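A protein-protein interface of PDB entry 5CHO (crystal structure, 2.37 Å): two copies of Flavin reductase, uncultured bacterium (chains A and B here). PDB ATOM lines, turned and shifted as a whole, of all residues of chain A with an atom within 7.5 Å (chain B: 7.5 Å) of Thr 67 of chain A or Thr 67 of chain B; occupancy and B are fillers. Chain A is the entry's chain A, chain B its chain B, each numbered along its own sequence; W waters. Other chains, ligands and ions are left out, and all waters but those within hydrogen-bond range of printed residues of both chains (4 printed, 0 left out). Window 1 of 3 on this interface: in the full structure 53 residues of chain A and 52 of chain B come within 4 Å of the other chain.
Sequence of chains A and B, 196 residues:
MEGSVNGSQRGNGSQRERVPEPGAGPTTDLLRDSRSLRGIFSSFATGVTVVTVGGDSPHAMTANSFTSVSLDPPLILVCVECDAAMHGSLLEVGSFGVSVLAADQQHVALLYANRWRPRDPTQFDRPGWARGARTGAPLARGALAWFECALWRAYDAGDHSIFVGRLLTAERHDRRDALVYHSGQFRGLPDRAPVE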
ATOM      1  N   PHE A  41      13.663 -20.417  -0.350  1.00  0.00           N
ATOM      2  CA  PHE A  41      13.713 -19.115  -1.018  1.00  0.00           C
ATOM      3  C   PHE A  41      12.592 -18.960  -2.045  1.00  0.00           C
ATOM      4  O   PHE A  41      12.078 -17.858  -2.237  1.00  0.00           O
ATOM      5  CB  PHE A  41      15.066 -18.900  -1.720  1.00  0.00           C
ATOM      6  CG  PHE A  41      16.230 -18.616  -0.790  1.00  0.00           C
ATOM      7  CD1 PHE A  41      16.036 -18.226   0.528  1.00  0.00           C
ATOM      8  CD2 PHE A  41      17.530 -18.726  -1.259  1.00  0.00           C
ATOM      9  CE1 PHE A  41      17.120 -17.963   1.354  1.00  0.00           C
ATOM     10  CE2 PHE A  41      18.612 -18.464  -0.440  1.00  0.00           C
ATOM     11  CZ  PHE A  41      18.407 -18.080   0.867  1.00  0.00           C
ATOM     12  N   PHE A  44       8.950 -17.190  -1.761  1.00  0.00           N
ATOM     13  CA  PHE A  44       8.738 -15.765  -2.015  1.00  0.00           C
ATOM     14  C   PHE A  44       8.620 -15.462  -3.505  1.00  0.00           C
ATOM     15  O   PHE A  44       9.599 -15.560  -4.245  1.00  0.00           O
ATOM     16  CB  PHE A  44       9.870 -14.933  -1.408  1.00  0.00           C
ATOM     17  CG  PHE A  44       9.635 -13.450  -1.485  1.00  0.00           C
ATOM     18  CD1 PHE A  44      10.213 -12.693  -2.495  1.00  0.00           C
ATOM     19  CD2 PHE A  44       8.845 -12.809  -0.544  1.00  0.00           C
ATOM     20  CE1 PHE A  44      10.002 -11.326  -2.565  1.00  0.00           C
ATOM     21  CE2 PHE A  44       8.626 -11.445  -0.614  1.00  0.00           C
ATOM     22  CZ  PHE A  44       9.209 -10.703  -1.624  1.00  0.00           C
ATOM     23  N   THR A  46       8.248 -13.488  -7.054  1.00  0.00           N
ATOM     24  CA  THR A  46       8.911 -12.326  -7.632  1.00  0.00           C
ATOM     25  C   THR A  46       8.425 -12.115  -9.051  1.00  0.00           C
ATOM     26  O   THR A  46       7.923 -13.039  -9.684  1.00  0.00           O
ATOM     27  CB  THR A  46      10.442 -12.481  -7.702  1.00  0.00           C
ATOM     28  OG1 THR A  46      10.767 -13.450  -8.704  1.00  0.00           O
ATOM     29  CG2 THR A  46      11.037 -12.909  -6.369  1.00  0.00           C
ATOM     30  N   THR A  49      13.076  -9.803 -14.348  1.00  0.00           N
ATOM     31  CA  THR A  49      13.698  -8.798 -15.214  1.00  0.00           C
ATOM     32  C   THR A  49      14.803  -9.361 -16.092  1.00  0.00           C
ATOM     33  O   THR A  49      15.278 -10.478 -15.890  1.00  0.00           O
ATOM     34  CB  THR A  49      14.326  -7.643 -14.409  1.00  0.00           C
ATOM     35  OG1 THR A  49      15.584  -8.068 -13.878  1.00  0.00           O
ATOM     36  CG2 THR A  49      13.429  -7.199 -13.272  1.00  0.00           C
ATOM     37  N   ASN A  64      15.853 -11.876 -11.003  1.00  0.00           N
ATOM     38  CA  ASN A  64      14.650 -11.640 -10.208  1.00  0.00           C
ATOM     39  C   ASN A  64      14.995 -11.032  -8.847  1.00  0.00           C
ATOM     40  O   ASN A  64      14.119 -10.839  -8.002  1.00  0.00           O
ATOM     41  CB  ASN A  64      13.850 -12.942 -10.035  1.00  0.00           C
ATOM     42  CG  ASN A  64      14.436 -13.869  -8.980  1.00  0.00           C
ATOM     43  OD1 ASN A  64      15.632 -13.830  -8.685  1.00  0.00           O
ATOM     44  ND2 ASN A  64      13.590 -14.733  -8.424  1.00  0.00           N
ATOM     45  N   SER A  65      16.275 -10.728  -8.647  1.00  0.00           N
ATOM     46  CA  SER A  65      16.732 -10.114  -7.404  1.00  0.00           C
ATOM     47  C   SER A  65      16.560  -8.596  -7.441  1.00  0.00           C
ATOM     48  O   SER A  65      17.018  -7.889  -6.542  1.00  0.00           O
ATOM     49  CB  SER A  65      18.199 -10.458  -7.141  1.00  0.00           C
ATOM     50  OG  SER A  65      19.030  -9.931  -8.161  1.00  0.00           O
ATOM     51  N   PHE A  66      15.906  -8.105  -8.488  1.00  0.00           N
ATOM     52  CA  PHE A  66      15.669  -6.678  -8.643  1.00  0.00           C
ATOM     53  C   PHE A  66      14.767  -6.165  -7.525  1.00  0.00           C
ATOM     54  O   PHE A  66      13.747  -6.774  -7.212  1.00  0.00           O
ATOM     55  CB  PHE A  66      15.046  -6.387 -10.007  1.00  0.00           C
ATOM     56  CG  PHE A  66      14.647  -4.948 -10.198  1.00  0.00           C
ATOM     57  CD1 PHE A  66      15.564  -4.006 -10.624  1.00  0.00           C
ATOM     58  CD2 PHE A  66      13.348  -4.542  -9.951  1.00  0.00           C
ATOM     59  CE1 PHE A  66      15.189  -2.687 -10.802  1.00  0.00           C
ATOM     60  CE2 PHE A  66      12.968  -3.227 -10.125  1.00  0.00           C
ATOM     61  CZ  PHE A  66      13.888  -2.297 -10.549  1.00  0.00           C
ATOM     62  N   THR A  67      15.159  -5.043  -6.927  1.00  0.00           N
ATOM     63  CA  THR A  67      14.458  -4.484  -5.773  1.00  0.00           C
ATOM     64  C   THR A  67      14.555  -2.960  -5.746  1.00  0.00           C
ATOM     65  O   THR A  67      15.640  -2.395  -5.865  1.00  0.00           O
ATOM     66  CB  THR A  67      15.012  -5.062  -4.452  1.00  0.00           C
ATOM     67  OG1 THR A  67      14.910  -6.493  -4.478  1.00  0.00           O
ATOM     68  CG2 THR A  67      14.236  -4.530  -3.254  1.00  0.00           C
ATOM     69  N   SER A  68      13.408  -2.307  -5.592  1.00  0.00           N
ATOM     70  CA  SER A  68      13.371  -0.859  -5.415  1.00  0.00           C
ATOM     71  C   SER A  68      13.894  -0.503  -4.029  1.00  0.00           C
ATOM     72  O   SER A  68      13.452  -1.076  -3.033  1.00  0.00           O
ATOM     73  CB  SER A  68      11.950  -0.330  -5.596  1.00  0.00           C
ATOM     74  OG  SER A  68      11.027  -1.074  -4.818  1.00  0.00           O
ATOM     75  N   VAL A  69      14.826   0.447  -3.964  1.00  0.00           N
ATOM     76  CA  VAL A  69      15.568   0.695  -2.728  1.00  0.00           C
ATOM     77  C   VAL A  69      15.288   2.062  -2.107  1.00  0.00           C
ATOM     78  O   VAL A  69      15.070   2.165  -0.901  1.00  0.00           O
ATOM     79  CB  VAL A  69      17.086   0.592  -2.961  1.00  0.00           C
ATOM     80  CG1 VAL A  69      17.834   0.992  -1.703  1.00  0.00           C
ATOM     81  CG2 VAL A  69      17.470  -0.817  -3.362  1.00  0.00           C
ATOM     82  N   SER A  70      15.295   3.106  -2.930  1.00  0.00           N
ATOM     83  CA  SER A  70      15.228   4.469  -2.424  1.00  0.00           C
ATOM     84  C   SER A  70      14.568   5.398  -3.433  1.00  0.00           C
ATOM     85  O   SER A  70      14.620   5.154  -4.638  1.00  0.00           O
ATOM     86  CB  SER A  70      16.633   4.972  -2.081  1.00  0.00           C
ATOM     87  OG  SER A  70      16.647   6.374  -1.887  1.00  0.00           O
ATOM     88  N   LEU A  75      17.082   5.011  -6.269  1.00  0.00           N
ATOM     89  CA  LEU A  75      18.005   3.884  -6.322  1.00  0.00           C
ATOM     90  C   LEU A  75      17.274   2.553  -6.482  1.00  0.00           C
ATOM     91  O   LEU A  75      16.149   2.390  -6.009  1.00  0.00           O
ATOM     92  CB  LEU A  75      18.858   3.833  -5.055  1.00  0.00           C
ATOM     93  CG  LEU A  75      19.810   4.972  -4.675  1.00  0.00           C
ATOM     94  CD1 LEU A  75      20.548   4.671  -3.389  1.00  0.00           C
ATOM     95  CD2 LEU A  75      20.786   5.268  -5.800  1.00  0.00           C
ATOM     96  N   ILE A  76      17.919   1.610  -7.164  1.00  0.00           N
ATOM     97  CA  ILE A  76      17.466   0.220  -7.194  1.00  0.00           C
ATOM     98  C   ILE A  76      18.662  -0.689  -6.947  1.00  0.00           C
ATOM     99  O   ILE A  76      19.801  -0.223  -6.942  1.00  0.00           O
ATOM    100  CB  ILE A  76      16.785  -0.152  -8.530  1.00  0.00           C
ATOM    101  CG1 ILE A  76      17.741   0.017  -9.718  1.00  0.00           C
ATOM    102  CG2 ILE A  76      15.545   0.698  -8.743  1.00  0.00           C
ATOM    103  CD1 ILE A  76      18.490  -1.246 -10.105  1.00  0.00           C
ATOM    104  N   LEU A  77      18.414  -1.977  -6.724  1.00  0.00           N
ATOM    105  CA  LEU A  77      19.512  -2.930  -6.636  1.00  0.00           C
ATOM    106  C   LEU A  77      19.200  -4.237  -7.346  1.00  0.00           C
ATOM    107  O   LEU A  77      18.041  -4.592  -7.554  1.00  0.00           O
ATOM    108  CB  LEU A  77      19.879  -3.197  -5.169  1.00  0.00           C
ATOM    109  CG  LEU A  77      18.964  -3.965  -4.213  1.00  0.00           C
ATOM    110  CD1 LEU A  77      18.926  -5.467  -4.502  1.00  0.00           C
ATOM    111  CD2 LEU A  77      19.438  -3.709  -2.792  1.00  0.00           C
ATOM    112  N   VAL A  78      20.264  -4.941  -7.715  1.00  0.00           N
ATOM    113  CA  VAL A  78      20.185  -6.305  -8.215  1.00  0.00           C
ATOM    114  C   VAL A  78      21.330  -7.092  -7.605  1.00  0.00           C
ATOM    115  O   VAL A  78      22.386  -6.526  -7.324  1.00  0.00           O
ATOM    116  CB  VAL A  78      20.284  -6.378  -9.754  1.00  0.00           C
ATOM    117  CG1 VAL A  78      19.079  -5.715 -10.413  1.00  0.00           C
ATOM    118  CG2 VAL A  78      21.583  -5.735 -10.239  1.00  0.00           C
ATOM    119  N   CYS A  79      21.122  -8.388  -7.391  1.00  0.00           N
ATOM    120  CA  CYS A  79      22.181  -9.248  -6.875  1.00  0.00           C
ATOM    121  C   CYS A  79      22.695 -10.150  -7.986  1.00  0.00           C
ATOM    122  O   CYS A  79      21.929 -10.902  -8.588  1.00  0.00           O
ATOM    123  CB  CYS A  79      21.683 -10.083  -5.700  1.00  0.00           C
ATOM    124  SG  CYS A  79      20.986  -9.099  -4.359  1.00  0.00           S
ATOM    125  N   VAL A  98      17.401  -2.269 -17.107  1.00  0.00           N
ATOM    126  CA  VAL A  98      16.551  -3.262 -16.471  1.00  0.00           C
ATOM    127  C   VAL A  98      15.189  -3.236 -17.150  1.00  0.00           C
ATOM    128  O   VAL A  98      14.585  -2.173 -17.280  1.00  0.00           O
ATOM    129  CB  VAL A  98      16.392  -2.984 -14.953  1.00  0.00           C
ATOM    130  CG1 VAL A  98      15.469  -4.004 -14.297  1.00  0.00           C
ATOM    131  CG2 VAL A  98      17.753  -2.952 -14.256  1.00  0.00           C
ATOM    132  N   PHE A 163      24.500  -4.876  -6.492  1.00  0.00           N
ATOM    133  CA  PHE A 163      24.776  -3.729  -7.347  1.00  0.00           C
ATOM    134  C   PHE A 163      23.673  -2.694  -7.182  1.00  0.00           C
ATOM    135  O   PHE A 163      22.536  -2.932  -7.578  1.00  0.00           O
ATOM    136  CB  PHE A 163      24.882  -4.149  -8.816  1.00  0.00           C
ATOM    137  CG  PHE A 163      26.096  -4.974  -9.128  1.00  0.00           C
ATOM    138  CD1 PHE A 163      26.116  -6.329  -8.861  1.00  0.00           C
ATOM    139  CD2 PHE A 163      27.220  -4.391  -9.685  1.00  0.00           C
ATOM    140  CE1 PHE A 163      27.232  -7.090  -9.148  1.00  0.00           C
ATOM    141  CE2 PHE A 163      28.337  -5.147  -9.975  1.00  0.00           C
ATOM    142  CZ  PHE A 163      28.342  -6.501  -9.703  1.00  0.00           C
ATOM    143  N   GLY A 165      22.065   0.751  -8.259  1.00  0.00           N
ATOM    144  CA  GLY A 165      22.048   1.667  -9.383  1.00  0.00           C
ATOM    145  C   GLY A 165      21.237   2.906  -9.080  1.00  0.00           C
ATOM    146  O   GLY A 165      20.132   2.809  -8.548  1.00  0.00           O
ATOM    147  N   PHE B  41       7.938   1.445 -10.200  1.00  0.00           N
ATOM    148  CA  PHE B  41       8.365   0.376  -9.302  1.00  0.00           C
ATOM    149  C   PHE B  41       7.309  -0.701  -9.101  1.00  0.00           C
ATOM    150  O   PHE B  41       7.648  -1.875  -8.966  1.00  0.00           O
ATOM    151  CB  PHE B  41       8.732   0.936  -7.923  1.00  0.00           C
ATOM    152  CG  PHE B  41      10.040   1.684  -7.867  1.00  0.00           C
ATOM    153  CD1 PHE B  41      11.002   1.566  -8.861  1.00  0.00           C
ATOM    154  CD2 PHE B  41      10.304   2.510  -6.788  1.00  0.00           C
ATOM    155  CE1 PHE B  41      12.198   2.259  -8.770  1.00  0.00           C
ATOM    156  CE2 PHE B  41      11.493   3.205  -6.695  1.00  0.00           C
ATOM    157  CZ  PHE B  41      12.439   3.082  -7.685  1.00  0.00           C
ATOM    158  N   PHE B  44       6.842  -4.234 -10.980  1.00  0.00           N
ATOM    159  CA  PHE B  44       7.545  -5.441 -10.546  1.00  0.00           C
ATOM    160  C   PHE B  44       6.846  -6.128  -9.373  1.00  0.00           C
ATOM    161  O   PHE B  44       6.832  -5.620  -8.250  1.00  0.00           O
ATOM    162  CB  PHE B  44       8.985  -5.115 -10.150  1.00  0.00           C
ATOM    163  CG  PHE B  44       9.814  -6.336  -9.825  1.00  0.00           C
ATOM    164  CD1 PHE B  44       9.922  -6.779  -8.519  1.00  0.00           C
ATOM    165  CD2 PHE B  44      10.459  -7.049 -10.818  1.00  0.00           C
ATOM    166  CE1 PHE B  44      10.670  -7.900  -8.207  1.00  0.00           C
ATOM    167  CE2 PHE B  44      11.210  -8.169 -10.511  1.00  0.00           C
ATOM    168  CZ  PHE B  44      11.313  -8.597  -9.204  1.00  0.00           C
ATOM    169  N   THR B  46       5.861  -8.765  -6.348  1.00  0.00           N
ATOM    170  CA  THR B  46       6.584  -9.331  -5.207  1.00  0.00           C
ATOM    171  C   THR B  46       5.698 -10.208  -4.341  1.00  0.00           C
ATOM    172  O   THR B  46       4.479 -10.090  -4.369  1.00  0.00           O
ATOM    173  CB  THR B  46       7.177  -8.232  -4.293  1.00  0.00           C
ATOM    174  OG1 THR B  46       6.111  -7.516  -3.655  1.00  0.00           O
ATOM    175  CG2 THR B  46       8.033  -7.259  -5.094  1.00  0.00           C
ATOM    176  N   THR B  49       6.314 -10.134   3.031  1.00  0.00           N
ATOM    177  CA  THR B  49       6.732 -10.638   4.327  1.00  0.00           C
ATOM    178  C   THR B  49       6.447  -9.703   5.482  1.00  0.00           C
ATOM    179  O   THR B  49       6.111  -8.531   5.298  1.00  0.00           O
ATOM    180  CB  THR B  49       8.237 -10.939   4.357  1.00  0.00           C
ATOM    181  OG1 THR B  49       8.967  -9.720   4.544  1.00  0.00           O
ATOM    182  CG2 THR B  49       8.664 -11.602   3.067  1.00  0.00           C
ATOM    183  N   ASN B  64       8.390  -6.014   1.426  1.00  0.00           N
ATOM    184  CA  ASN B  64       8.423  -6.761   0.174  1.00  0.00           C
ATOM    185  C   ASN B  64       9.772  -6.600  -0.530  1.00  0.00           C
ATOM    186  O   ASN B  64       9.953  -7.050  -1.664  1.00  0.00           O
ATOM    187  CB  ASN B  64       7.264  -6.336  -0.734  1.00  0.00           C
ATOM    188  CG  ASN B  64       7.499  -5.003  -1.409  1.00  0.00           C
ATOM    189  OD1 ASN B  64       8.237  -4.161  -0.902  1.00  0.00           O
ATOM    190  ND2 ASN B  64       6.874  -4.808  -2.568  1.00  0.00           N
ATOM    191  N   SER B  65      10.713  -5.942   0.146  1.00  0.00           N
ATOM    192  CA  SER B  65      12.063  -5.775  -0.375  1.00  0.00           C
ATOM    193  C   SER B  65      12.911  -7.001  -0.045  1.00  0.00           C
ATOM    194  O   SER B  65      14.119  -7.001  -0.277  1.00  0.00           O
ATOM    195  CB  SER B  65      12.718  -4.522   0.209  1.00  0.00           C
ATOM    196  OG  SER B  65      12.851  -4.627   1.615  1.00  0.00           O
ATOM    197  N   PHE B  66      12.277  -8.038   0.498  1.00  0.00           N
ATOM    198  CA  PHE B  66      12.979  -9.261   0.856  1.00  0.00           C
ATOM    199  C   PHE B  66      13.524  -9.927  -0.401  1.00  0.00           C
ATOM    200  O   PHE B  66      12.825 -10.062  -1.404  1.00  0.00           O
ATOM    201  CB  PHE B  66      12.058 -10.213   1.620  1.00  0.00           C
ATOM    202  CG  PHE B  66      12.676 -11.552   1.918  1.00  0.00           C
ATOM    203  CD1 PHE B  66      13.508 -11.718   3.013  1.00  0.00           C
ATOM    204  CD2 PHE B  66      12.400 -12.649   1.123  1.00  0.00           C
ATOM    205  CE1 PHE B  66      14.071 -12.947   3.296  1.00  0.00           C
ATOM    206  CE2 PHE B  66      12.961 -13.886   1.400  1.00  0.00           C
ATOM    207  CZ  PHE B  66      13.798 -14.033   2.489  1.00  0.00           C
ATOM    208  N   THR B  67      14.786 -10.334  -0.334  1.00  0.00           N
ATOM    209  CA  THR B  67      15.485 -10.863  -1.496  1.00  0.00           C
ATOM    210  C   THR B  67      16.505 -11.915  -1.079  1.00  0.00           C
ATOM    211  O   THR B  67      17.312 -11.678  -0.184  1.00  0.00           O
ATOM    212  CB  THR B  67      16.200  -9.736  -2.265  1.00  0.00           C
ATOM    213  OG1 THR B  67      15.264  -8.701  -2.589  1.00  0.00           O
ATOM    214  CG2 THR B  67      16.844 -10.262  -3.540  1.00  0.00           C
ATOM    215  N   SER B  68      16.463 -13.078  -1.721  1.00  0.00           N
ATOM    216  CA  SER B  68      17.490 -14.097  -1.518  1.00  0.00           C
ATOM    217  C   SER B  68      18.779 -13.632  -2.179  1.00  0.00           C
ATOM    218  O   SER B  68      18.766 -13.211  -3.336  1.00  0.00           O
ATOM    219  CB  SER B  68      17.049 -15.444  -2.091  1.00  0.00           C
ATOM    220  OG  SER B  68      16.568 -15.298  -3.417  1.00  0.00           O
ATOM    221  N   VAL B  69      19.885 -13.708  -1.446  1.00  0.00           N
ATOM    222  CA  VAL B  69      21.132 -13.075  -1.879  1.00  0.00           C
ATOM    223  C   VAL B  69      22.247 -14.070  -2.206  1.00  0.00           C
ATOM    224  O   VAL B  69      22.907 -13.950  -3.238  1.00  0.00           O
ATOM    225  CB  VAL B  69      21.645 -12.100  -0.801  1.00  0.00           C
ATOM    226  CG1 VAL B  69      23.041 -11.605  -1.140  1.00  0.00           C
ATOM    227  CG2 VAL B  69      20.681 -10.937  -0.648  1.00  0.00           C
ATOM    228  N   SER B  70      22.452 -15.047  -1.331  1.00  0.00           N
ATOM    229  CA  SER B  70      23.592 -15.945  -1.454  1.00  0.00           C
ATOM    230  C   SER B  70      23.275 -17.299  -0.830  1.00  0.00           C
ATOM    231  O   SER B  70      22.444 -17.386   0.074  1.00  0.00           O
ATOM    232  CB  SER B  70      24.829 -15.328  -0.792  1.00  0.00           C
ATOM    233  OG  SER B  70      25.865 -16.284  -0.627  1.00  0.00           O
ATOM    234  N   LEU B  75      22.552 -16.104   2.555  1.00  0.00           N
ATOM    235  CA  LEU B  75      22.226 -14.710   2.860  1.00  0.00           C
ATOM    236  C   LEU B  75      20.900 -14.255   2.248  1.00  0.00           C
ATOM    237  O   LEU B  75      20.499 -14.722   1.182  1.00  0.00           O
ATOM    238  CB  LEU B  75      23.320 -13.764   2.355  1.00  0.00           C
ATOM    239  CG  LEU B  75      24.759 -13.884   2.861  1.00  0.00           C
ATOM    240  CD1 LEU B  75      25.621 -12.789   2.235  1.00  0.00           C
ATOM    241  CD2 LEU B  75      24.820 -13.828   4.375  1.00  0.00           C
ATOM    242  N   ILE B  76      20.231 -13.340   2.944  1.00  0.00           N
ATOM    243  CA  ILE B  76      19.086 -12.613   2.403  1.00  0.00           C
ATOM    244  C   ILE B  76      19.252 -11.127   2.720  1.00  0.00           C
ATOM    245  O   ILE B  76      20.114 -10.757   3.517  1.00  0.00           O
ATOM    246  CB  ILE B  76      17.752 -13.117   2.982  1.00  0.00           C
ATOM    247  CG1 ILE B  76      17.701 -12.895   4.496  1.00  0.00           C
ATOM    248  CG2 ILE B  76      17.561 -14.583   2.648  1.00  0.00           C
ATOM    249  CD1 ILE B  76      17.061 -11.578   4.907  1.00  0.00           C
ATOM    250  N   LEU B  77      18.438 -10.276   2.105  1.00  0.00           N
ATOM    251  CA  LEU B  77      18.431  -8.863   2.474  1.00  0.00           C
ATOM    252  C   LEU B  77      17.022  -8.289   2.497  1.00  0.00           C
ATOM    253  O   LEU B  77      16.125  -8.816   1.847  1.00  0.00           O
ATOM    254  CB  LEU B  77      19.331  -8.061   1.519  1.00  0.00           C
ATOM    255  CG  LEU B  77      18.917  -7.854   0.051  1.00  0.00           C
ATOM    256  CD1 LEU B  77      17.812  -6.814  -0.100  1.00  0.00           C
ATOM    257  CD2 LEU B  77      20.120  -7.496  -0.822  1.00  0.00           C
ATOM    258  N   VAL B  78      16.850  -7.200   3.245  1.00  0.00           N
ATOM    259  CA  VAL B  78      15.629  -6.399   3.220  1.00  0.00           C
ATOM    260  C   VAL B  78      16.049  -4.940   3.218  1.00  0.00           C
ATOM    261  O   VAL B  78      17.101  -4.596   3.759  1.00  0.00           O
ATOM    262  CB  VAL B  78      14.713  -6.639   4.444  1.00  0.00           C
ATOM    263  CG1 VAL B  78      14.182  -8.074   4.468  1.00  0.00           C
ATOM    264  CG2 VAL B  78      15.458  -6.317   5.733  1.00  0.00           C
ATOM    265  N   CYS B  79      15.240  -4.086   2.606  1.00  0.00           N
ATOM    266  CA  CYS B  79      15.514  -2.655   2.596  1.00  0.00           C
ATOM    267  C   CYS B  79      14.549  -1.942   3.526  1.00  0.00           C
ATOM    268  O   CYS B  79      13.335  -2.061   3.376  1.00  0.00           O
ATOM    269  CB  CYS B  79      15.414  -2.098   1.182  1.00  0.00           C
ATOM    270  SG  CYS B  79      16.515  -2.928   0.014  1.00  0.00           S
ATOM    271  N   PHE B 163      19.702  -4.177   4.713  1.00  0.00           N
ATOM    272  CA  PHE B 163      20.068  -5.041   5.829  1.00  0.00           C
ATOM    273  C   PHE B 163      20.295  -6.453   5.313  1.00  0.00           C
ATOM    274  O   PHE B 163      19.350  -7.115   4.898  1.00  0.00           O
ATOM    275  CB  PHE B 163      18.981  -5.046   6.911  1.00  0.00           C
ATOM    276  CG  PHE B 163      18.873  -3.756   7.677  1.00  0.00           C
ATOM    277  CD1 PHE B 163      18.181  -2.678   7.155  1.00  0.00           C
ATOM    278  CD2 PHE B 163      19.466  -3.625   8.921  1.00  0.00           C
ATOM    279  CE1 PHE B 163      18.085  -1.492   7.860  1.00  0.00           C
ATOM    280  CE2 PHE B 163      19.370  -2.443   9.632  1.00  0.00           C
ATOM    281  CZ  PHE B 163      18.680  -1.376   9.100  1.00  0.00           C
ATOM    282  N   GLY B 165      21.134 -10.262   6.026  1.00  0.00           N
ATOM    283  CA  GLY B 165      21.059 -11.248   7.091  1.00  0.00           C
ATOM    284  C   GLY B 165      21.630 -12.594   6.683  1.00  0.00           C
ATOM    285  O   GLY B 165      21.338 -13.094   5.598  1.00  0.00           O
HETATM  286  O   HOH W   1      13.544  -9.186  -5.215  1.00  0.00           O
HETATM  287  O   HOH W   2      16.295 -13.379  -5.762  1.00  0.00           O
HETATM  288  O   HOH W   3      11.928  -7.765  -3.592  1.00  0.00           O
HETATM  289  O   HOH W   4      13.415 -15.575  -3.652  1.00  0.00           O
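The side-chain hydroxyl (OG1) of Thr 67 of chain B lies within hydrogen-bond range of the side-chain hydroxyl (OG1) of Thr 67 of chain A.
The side-chain hydroxyl (OG) of Ser 65 of chain A lies within hydrogen-bond range of the backbone NH (N) of Cys 79 of chain A (2.7 Å).
The backbone carbonyl oxygen (O) of Thr 67 of chain A sits at hydrogen-bond distance from the backbone NH (N) of Leu 77 of chain A (2.9 Å).
ND2 of Asn 64 of chain B sits at hydrogen-bond distance from OG1 of Thr 46 of chain B, at 3.0 Å.
The side-chain hydroxyl (OG) of Ser 65 of chain B lies within hydrogen-bond range of the backbone NH (N) of Cys 79 of chain B (2.6 Å).
O of Leu 75 of chain B lies within hydrogen-bond range of N of Val 69 of chain B (2.9 Å).
Among the printed residues, pairs that only touch across the chains: Phe 44 of chain A with Phe 66 of chain B (3.3 Å), Phe 41 of chain A with Ser 68 of chain B (3.4 Å), Phe 66 of chain A with Phe 44 of chain B (3.4 Å), Ser 68 of chain A with Phe 41 of chain B (3.5 Å), Phe 41 of chain A with Ile 76 of chain B (3.6 Å), Thr 49 of chain A with Phe 44 of chain B (3.7 Å), Phe 44 of chain A with Thr 49 of chain B (3.7 Å), Ile 76 of chain A with Phe 41 of chain B (3.7 Å), Phe 44 of chain A with Asn 64 of chain B (3.7 Å), Thr 67 of chain A with Ser 65 of chain B (3.8 Å), Asn 64 of chain A with Phe 44 of chain B (3.8 Å), Ser 65 of chain A with Thr 67 of chain B (3.8 Å), Phe 41 of chain A with Leu 75 of chain B (3.97 Å) and Cys 79 of chain A with Leu 77 of chain B (3.98 Å).
Thr 67 of chain A touches two residues of chain B.
Of the printed residues of chain A, Thr 67 of chain B touches Ser 65 (3.8 Å) and Thr 67 (2.9 Å).
Of the printed residues of chain A, Phe 66 of chain B touches Phe 44.
Of the printed residues of chain A, Phe 41 of chain B touches Ser 68 (3.5 Å) and Ile 76 (3.7 Å).
Of the printed residues of chain A, Asn 64 of chain B touches Phe 44 (3.7 Å).
Of the printed residues of chain B, Phe 41 of chain A touches Ser 68 (3.4 Å), Leu 75 (3.97 Å) and Ile 76 (3.6 Å).
Printed residues of chain A within 4 Å of Leu 75 of chain B: Phe 41 (3.97 Å).
The nearest residue of chain B that does not touch Thr 67 of chain A is Cys 79 of chain B (4.3 Å).
The nearest residue of chain A that does not touch Thr 67 of chain B is Cys 79 of chain A (4.4 Å).
The nearest printed residue of chain A that does not touch Phe 66 of chain B is Phe 41 of chain A (5.1 Å).
Of the 18 printed residues of chain B, 11 touch a printed residue of chain A.
Hydrophobic or aromatic side chains of chain B within 4 Å of the printed part of chain A: Phe 41, Phe 44, Phe 66, Ile 76 and Leu 77.
Of the 19 printed residues of chain A, 10 touch a printed residue of chain B.
Among the printed residues, 15 pairs touch across the chains.
Phe 41 of chain A touches Ser 68 of chain B, and with the chains exchanged Ser 68 of chain A touches Phe 41 of chain B.
Ser 65 of chain A touches Thr 67 of chain B, and with the chains exchanged Thr 67 of chain A touches Ser 65 of chain B.
Thr 67 of chain B touches its own counterpart, Thr 67 of chain A.
Cys 79 of chain A touches Leu 77 of chain B, but with the chains exchanged Leu 77 of chain A does not touch Cys 79 of chain B (4.1 Å).
Positions printed for both chains: 41, 44, 46, 49, 64, 65, 66, 67, 68, 69, 70, 75, 76, 77, 78, 79, 163 and 165.
Of the 15 pairs that touch across the chains among the printed residues, 13 have their exchanged pair printed and touching as well.
Water W3 lies within hydrogen-bond range of the backbone carbonyl oxygen (O) of Asn 64 of chain B, the backbone carbonyl oxygen (O) of Phe 66 of chain B and the side-chain hydroxyl (OG1) of Thr 67 of chain A.
Water W4 bridges the backbone carbonyl oxygen (O) of Phe 41 of chain A and the side-chain hydroxyl (OG) of Ser 68 of chain B.
Water W2 bridges the side-chain amide oxygen (OD1) of Asn 64 of chain A and the side-chain hydroxyl (OG) of Ser 68 of chain B.
Water W1 lies within hydrogen-bond range of OG1 of Thr 67 of chain A (3.1 Å), O of Phe 66 of chain A (3.1 Å), OG1 of Thr 67 of chain B (3.2 Å) and O of Asn 64 of chain A (3.3 Å).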
